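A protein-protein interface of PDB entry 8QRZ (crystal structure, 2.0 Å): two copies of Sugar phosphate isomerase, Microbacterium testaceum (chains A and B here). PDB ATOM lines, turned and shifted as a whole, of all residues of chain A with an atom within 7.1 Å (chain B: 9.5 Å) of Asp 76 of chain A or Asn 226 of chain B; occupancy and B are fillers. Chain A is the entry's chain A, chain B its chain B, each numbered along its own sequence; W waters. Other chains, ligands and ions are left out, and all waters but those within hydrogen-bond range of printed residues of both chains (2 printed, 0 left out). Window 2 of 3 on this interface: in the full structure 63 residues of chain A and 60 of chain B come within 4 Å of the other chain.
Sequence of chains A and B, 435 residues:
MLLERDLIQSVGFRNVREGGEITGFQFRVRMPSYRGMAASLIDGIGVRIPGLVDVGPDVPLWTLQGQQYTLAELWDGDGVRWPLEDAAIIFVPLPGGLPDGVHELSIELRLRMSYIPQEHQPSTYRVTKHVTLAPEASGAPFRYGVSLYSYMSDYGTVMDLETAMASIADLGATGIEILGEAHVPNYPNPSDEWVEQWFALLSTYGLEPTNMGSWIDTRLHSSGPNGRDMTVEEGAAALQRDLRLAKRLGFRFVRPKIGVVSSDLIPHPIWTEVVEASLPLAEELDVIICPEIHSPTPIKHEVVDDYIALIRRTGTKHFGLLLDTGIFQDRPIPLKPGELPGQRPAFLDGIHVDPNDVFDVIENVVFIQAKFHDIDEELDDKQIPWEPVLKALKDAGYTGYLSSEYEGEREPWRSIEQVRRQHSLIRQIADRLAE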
ATOM      1  N   SER A  40     -25.499 -19.821 -15.819  1.00  0.00           N
ATOM      2  CA  SER A  40     -25.958 -20.190 -14.490  1.00  0.00           C
ATOM      3  C   SER A  40     -27.066 -21.231 -14.509  1.00  0.00           C
ATOM      4  O   SER A  40     -27.378 -21.787 -13.452  1.00  0.00           O
ATOM      5  CB  SER A  40     -26.431 -18.943 -13.755  1.00  0.00           C
ATOM      6  OG  SER A  40     -27.462 -18.317 -14.472  1.00  0.00           O
ATOM      7  N   LEU A  71     -18.554 -25.052 -11.012  1.00  0.00           N
ATOM      8  CA  LEU A  71     -20.009 -25.011 -11.053  1.00  0.00           C
ATOM      9  C   LEU A  71     -20.558 -24.019 -10.039  1.00  0.00           C
ATOM     10  O   LEU A  71     -21.566 -23.354 -10.300  1.00  0.00           O
ATOM     11  CB  LEU A  71     -20.609 -26.387 -10.798  1.00  0.00           C
ATOM     12  CG  LEU A  71     -22.139 -26.462 -10.924  1.00  0.00           C
ATOM     13  CD1 LEU A  71     -22.647 -26.080 -12.342  1.00  0.00           C
ATOM     14  CD2 LEU A  71     -22.647 -27.836 -10.497  1.00  0.00           C
ATOM     15  N   ALA A  72     -19.936 -23.927  -8.860  1.00  0.00           N
ATOM     16  CA  ALA A  72     -20.441 -22.980  -7.871  1.00  0.00           C
ATOM     17  C   ALA A  72     -20.393 -21.571  -8.437  1.00  0.00           C
ATOM     18  O   ALA A  72     -21.319 -20.772  -8.229  1.00  0.00           O
ATOM     19  CB  ALA A  72     -19.643 -23.087  -6.564  1.00  0.00           C
ATOM     20  N   GLU A  73     -19.356 -21.277  -9.229  1.00  0.00           N
ATOM     21  CA  GLU A  73     -19.250 -19.959  -9.835  1.00  0.00           C
ATOM     22  C   GLU A  73     -20.315 -19.758 -10.903  1.00  0.00           C
ATOM     23  O   GLU A  73     -21.012 -18.742 -10.902  1.00  0.00           O
ATOM     24  CB  GLU A  73     -17.852 -19.762 -10.396  1.00  0.00           C
ATOM     25  CG  GLU A  73     -16.888 -19.444  -9.289  1.00  0.00           C
ATOM     26  CD  GLU A  73     -15.470 -19.626  -9.685  1.00  0.00           C
ATOM     27  OE1 GLU A  73     -15.201 -20.312 -10.697  1.00  0.00           O
ATOM     28  OE2 GLU A  73     -14.612 -19.074  -8.984  1.00  0.00           O
ATOM     29  N   LEU A  74     -20.469 -20.722 -11.811  1.00  0.00           N
ATOM     30  CA  LEU A  74     -21.547 -20.642 -12.790  1.00  0.00           C
ATOM     31  C   LEU A  74     -22.890 -20.337 -12.124  1.00  0.00           C
ATOM     32  O   LEU A  74     -23.648 -19.490 -12.601  1.00  0.00           O
ATOM     33  CB  LEU A  74     -21.619 -21.942 -13.582  1.00  0.00           C
ATOM     34  CG  LEU A  74     -20.489 -22.234 -14.577  1.00  0.00           C
ATOM     35  CD1 LEU A  74     -20.983 -23.320 -15.496  1.00  0.00           C
ATOM     36  CD2 LEU A  74     -20.074 -21.015 -15.380  1.00  0.00           C
ATOM     37  N   TRP A  75     -23.172 -20.961 -10.980  1.00  0.00           N
ATOM     38  CA  TRP A  75     -24.471 -20.750 -10.341  1.00  0.00           C
ATOM     39  C   TRP A  75     -24.691 -19.288  -9.956  1.00  0.00           C
ATOM     40  O   TRP A  75     -25.803 -18.764 -10.114  1.00  0.00           O
ATOM     41  CB  TRP A  75     -24.622 -21.660  -9.122  1.00  0.00           C
ATOM     42  CG  TRP A  75     -25.060 -23.033  -9.528  1.00  0.00           C
ATOM     43  CD1 TRP A  75     -25.618 -23.386 -10.719  1.00  0.00           C
ATOM     44  CD2 TRP A  75     -24.974 -24.227  -8.750  1.00  0.00           C
ATOM     45  NE1 TRP A  75     -25.886 -24.733 -10.738  1.00  0.00           N
ATOM     46  CE2 TRP A  75     -25.500 -25.271  -9.532  1.00  0.00           C
ATOM     47  CE3 TRP A  75     -24.499 -24.517  -7.462  1.00  0.00           C
ATOM     48  CZ2 TRP A  75     -25.567 -26.594  -9.066  1.00  0.00           C
ATOM     49  CZ3 TRP A  75     -24.570 -25.822  -7.004  1.00  0.00           C
ATOM     50  CH2 TRP A  75     -25.095 -26.845  -7.802  1.00  0.00           C
ATOM     51  N   ASP A  76     -23.642 -18.604  -9.502  1.00  0.00           N
ATOM     52  CA  ASP A  76     -23.757 -17.225  -9.045  1.00  0.00           C
ATOM     53  C   ASP A  76     -23.422 -16.193 -10.116  1.00  0.00           C
ATOM     54  O   ASP A  76     -23.605 -14.997  -9.871  1.00  0.00           O
ATOM     55  CB  ASP A  76     -22.870 -16.993  -7.817  1.00  0.00           C
ATOM     56  CG  ASP A  76     -23.330 -17.798  -6.600  1.00  0.00           C
ATOM     57  OD1 ASP A  76     -24.379 -18.469  -6.702  1.00  0.00           O
ATOM     58  OD2 ASP A  76     -22.662 -17.749  -5.541  1.00  0.00           O
ATOM     59  N   GLY A  77     -22.977 -16.618 -11.302  1.00  0.00           N
ATOM     60  CA  GLY A  77     -22.585 -15.674 -12.327  1.00  0.00           C
ATOM     61  C   GLY A  77     -23.768 -15.032 -13.037  1.00  0.00           C
ATOM     62  O   GLY A  77     -24.860 -15.580 -13.103  1.00  0.00           O
ATOM     63  N   ASP A  78     -23.529 -13.839 -13.584  1.00  0.00           N
ATOM     64  CA  ASP A  78     -24.478 -13.117 -14.426  1.00  0.00           C
ATOM     65  C   ASP A  78     -23.790 -12.769 -15.741  1.00  0.00           C
ATOM     66  O   ASP A  78     -22.616 -12.386 -15.754  1.00  0.00           O
ATOM     67  CB  ASP A  78     -24.953 -11.814 -13.747  1.00  0.00           C
ATOM     68  CG  ASP A  78     -26.289 -11.961 -13.024  1.00  0.00           C
ATOM     69  OD1 ASP A  78     -27.293 -12.335 -13.648  1.00  0.00           O
ATOM     70  OD2 ASP A  78     -26.325 -11.712 -11.801  1.00  0.00           O
ATOM     71  N   LEU B 220     -33.181 -18.661 -13.428  1.00  0.00           N
ATOM     72  CA  LEU B 220     -31.804 -18.241 -13.681  1.00  0.00           C
ATOM     73  C   LEU B 220     -30.830 -18.580 -12.558  1.00  0.00           C
ATOM     74  O   LEU B 220     -29.774 -19.165 -12.811  1.00  0.00           O
ATOM     75  CB  LEU B 220     -31.778 -16.736 -13.960  1.00  0.00           C
ATOM     76  CG  LEU B 220     -30.456 -16.287 -14.598  1.00  0.00           C
ATOM     77  CD1 LEU B 220     -30.216 -17.066 -15.875  1.00  0.00           C
ATOM     78  CD2 LEU B 220     -30.394 -14.787 -14.852  1.00  0.00           C
ATOM     79  N   HIS B 221     -31.133 -18.196 -11.312  1.00  0.00           N
ATOM     80  CA  HIS B 221     -30.236 -18.585 -10.229  1.00  0.00           C
ATOM     81  C   HIS B 221     -30.959 -19.386  -9.147  1.00  0.00           C
ATOM     82  O   HIS B 221     -30.902 -19.032  -7.966  1.00  0.00           O
ATOM     83  CB  HIS B 221     -29.555 -17.377  -9.586  1.00  0.00           C
ATOM     84  CG  HIS B 221     -28.878 -16.456 -10.551  1.00  0.00           C
ATOM     85  ND1 HIS B 221     -29.529 -15.407 -11.157  1.00  0.00           N
ATOM     86  CD2 HIS B 221     -27.599 -16.404 -10.984  1.00  0.00           C
ATOM     87  CE1 HIS B 221     -28.686 -14.761 -11.941  1.00  0.00           C
ATOM     88  NE2 HIS B 221     -27.509 -15.348 -11.856  1.00  0.00           N
ATOM     89  N   SER B 222     -31.622 -20.471  -9.542  1.00  0.00           N
ATOM     90  CA  SER B 222     -32.362 -21.333  -8.627  1.00  0.00           C
ATOM     91  C   SER B 222     -31.489 -22.353  -7.892  1.00  0.00           C
ATOM     92  O   SER B 222     -31.990 -23.024  -6.983  1.00  0.00           O
ATOM     93  CB  SER B 222     -33.469 -22.061  -9.390  1.00  0.00           C
ATOM     94  OG  SER B 222     -32.992 -23.260  -9.991  1.00  0.00           O
ATOM     95  N   SER B 223     -30.207 -22.483  -8.221  1.00  0.00           N
ATOM     96  CA  SER B 223     -29.369 -23.504  -7.601  1.00  0.00           C
ATOM     97  C   SER B 223     -28.277 -22.870  -6.749  1.00  0.00           C
ATOM     98  O   SER B 223     -27.946 -21.695  -6.904  1.00  0.00           O
ATOM     99  CB  SER B 223     -28.739 -24.405  -8.664  1.00  0.00           C
ATOM    100  OG  SER B 223     -29.695 -24.700  -9.660  1.00  0.00           O
ATOM    101  N   GLY B 224     -27.726 -23.663  -5.834  1.00  0.00           N
ATOM    102  CA  GLY B 224     -26.598 -23.239  -5.039  1.00  0.00           C
ATOM    103  C   GLY B 224     -26.996 -22.597  -3.728  1.00  0.00           C
ATOM    104  O   GLY B 224     -28.179 -22.380  -3.447  1.00  0.00           O
ATOM    105  N   PRO B 225     -26.005 -22.267  -2.897  1.00  0.00           N
ATOM    106  CA  PRO B 225     -26.339 -21.732  -1.567  1.00  0.00           C
ATOM    107  C   PRO B 225     -26.912 -20.339  -1.647  1.00  0.00           C
ATOM    108  O   PRO B 225     -27.731 -19.950  -0.801  1.00  0.00           O
ATOM    109  CB  PRO B 225     -24.995 -21.748  -0.825  1.00  0.00           C
ATOM    110  CG  PRO B 225     -23.911 -21.795  -1.921  1.00  0.00           C
ATOM    111  CD  PRO B 225     -24.574 -22.102  -3.240  1.00  0.00           C
ATOM    112  N   ASN B 226     -26.504 -19.581  -2.658  1.00  0.00           N
ATOM    113  CA  ASN B 226     -26.905 -18.192  -2.817  1.00  0.00           C
ATOM    114  C   ASN B 226     -28.066 -18.085  -3.785  1.00  0.00           C
ATOM    115  O   ASN B 226     -28.172 -17.137  -4.569  1.00  0.00           O
ATOM    116  CB  ASN B 226     -25.712 -17.358  -3.270  1.00  0.00           C
ATOM    117  CG  ASN B 226     -25.480 -16.153  -2.378  1.00  0.00           C
ATOM    118  OD1 ASN B 226     -26.327 -15.815  -1.541  1.00  0.00           O
ATOM    119  ND2 ASN B 226     -24.315 -15.519  -2.520  1.00  0.00           N
ATOM    120  N   GLY B 227     -28.954 -19.074  -3.736  1.00  0.00           N
ATOM    121  CA  GLY B 227     -30.079 -19.093  -4.647  1.00  0.00           C
ATOM    122  C   GLY B 227     -31.008 -17.916  -4.429  1.00  0.00           C
ATOM    123  O   GLY B 227     -31.164 -17.409  -3.314  1.00  0.00           O
ATOM    124  N   ARG B 228     -31.630 -17.482  -5.520  1.00  0.00           N
ATOM    125  CA  ARG B 228     -32.562 -16.369  -5.490  1.00  0.00           C
ATOM    126  C   ARG B 228     -33.595 -16.572  -6.583  1.00  0.00           C
ATOM    127  O   ARG B 228     -33.548 -17.544  -7.340  1.00  0.00           O
ATOM    128  CB  ARG B 228     -31.831 -15.044  -5.657  1.00  0.00           C
ATOM    129  CG  ARG B 228     -31.124 -14.888  -6.988  1.00  0.00           C
ATOM    130  CD  ARG B 228     -30.591 -13.486  -7.051  1.00  0.00           C
ATOM    131  NE  ARG B 228     -29.809 -13.203  -8.246  1.00  0.00           N
ATOM    132  CZ  ARG B 228     -28.519 -13.472  -8.361  1.00  0.00           C
ATOM    133  NH1 ARG B 228     -27.860 -14.107  -7.401  1.00  0.00           N
ATOM    134  NH2 ARG B 228     -27.870 -13.089  -9.461  1.00  0.00           N
ATOM    135  N   ASP B 229     -34.528 -15.640  -6.673  1.00  0.00           N
ATOM    136  CA  ASP B 229     -35.579 -15.720  -7.667  1.00  0.00           C
ATOM    137  C   ASP B 229     -35.469 -14.522  -8.599  1.00  0.00           C
ATOM    138  O   ASP B 229     -34.817 -13.530  -8.279  1.00  0.00           O
ATOM    139  CB  ASP B 229     -36.957 -15.777  -7.004  1.00  0.00           C
ATOM    140  CG  ASP B 229     -37.788 -16.930  -7.507  1.00  0.00           C
ATOM    141  OD1 ASP B 229     -38.633 -17.425  -6.731  1.00  0.00           O
ATOM    142  OD2 ASP B 229     -37.589 -17.340  -8.677  1.00  0.00           O
HETATM  143  O   HOH W   1     -26.829 -16.040 -15.121  1.00  0.00           O
HETATM  144  O   HOH W   2     -28.217 -20.741  -9.780  1.00  0.00           O
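The backbone carbonyl oxygen (O) of Leu 220 of chain B is in hydrogen-bond range of the side-chain hydroxyl (OG) of Ser 40 of chain A.
A ring nitrogen (NE2) of His 221 of chain B sits at hydrogen-bond distance from the backbone carbonyl oxygen of Gly 77 of chain A (2.9 Å).
The guanidinium group (NH2) of Arg 228 of chain B is in salt-bridge range of the side-chain carboxylate (OD2) of Asp 78 of chain A (3.1 Å).
The backbone carbonyl oxygen (O) of His 221 of chain B sits at hydrogen-bond distance from the backbone NH (N) of Arg 228 of chain B (3.0 Å).
CB of Ser 40 of chain A touches CD2 of His 221 of chain B, at 3.9 Å.
His 221 of chain B touches Trp 75 of chain A (CD2 to O, 3.1 Å).
Trp 75 of chain A touches Ser 223 of chain B (CE2 to CB, 3.5 Å).
Gly 224 of chain B touches Trp 75 of chain A (CA to CE3, 3.5 Å).
Asp 76 of chain A touches Asn 226 of chain B (OD2 to CB, 3.8 Å).
CE1 of His 221 of chain B touches OD1 of Asp 78 of chain A (3.3 Å).
Asp 76 of chain A touches just one residue of chain B: Asn 226 (3.8 Å).
Of chain A, only Asp 76 (3.8 Å) comes within 4 Å of Asn 226 of chain B.
Gly 77 of chain A touches just one residue of chain B: His 221.
Of the printed residues of chain B, Asp 78 of chain A touches His 221 and Arg 228.
Of the printed residues of chain B, Ser 40 of chain A touches Leu 220 and His 221.
Gly 227 of chain B touches none of the printed residues of chain A.
Glu 73 of chain A touches none of the printed residues of chain B.
The nearest residue of chain A that does not touch Asn 226 of chain B is Trp 75 of chain A (6.2 Å).
The nearest printed residue of chain A that does not touch Leu 220 of chain B is Asp 78 of chain A (4.1 Å).
Along chain B the printed residues that touch a printed residue of chain A span positions 220 to 228.
Of the 9 printed residues of chain A, 5 touch a printed residue of chain B.
Hydrophobic or aromatic side chains of chain A that line the printed part of chain B: Trp 75.
Among the printed residues, 9 pairs touch across the chains.
Among the printed residues, Asp or Glu carboxylates within 4 Å of a Lys or Arg side-chain nitrogen of the other chain: Asp 78 of chain A with Arg 228 of chain B (3.1 Å).
No position is printed for both chains.
Of the 9 pairs that touch across the chains among the printed residues, none has its exchanged pair printed and touching as well.
Water W1 lies within hydrogen-bond range of OG of Ser 40 of chain A (2.5 Å), O of Gly 77 of chain A (2.9 Å) and NE2 of His 221 of chain B (3.4 Å).
Water W2 lies within hydrogen-bond range of O of Ser 223 of chain B (3.0 Å), O of Trp 75 of chain A (3.1 Å) and N of Ser 222 of chain B (3.4 Å).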
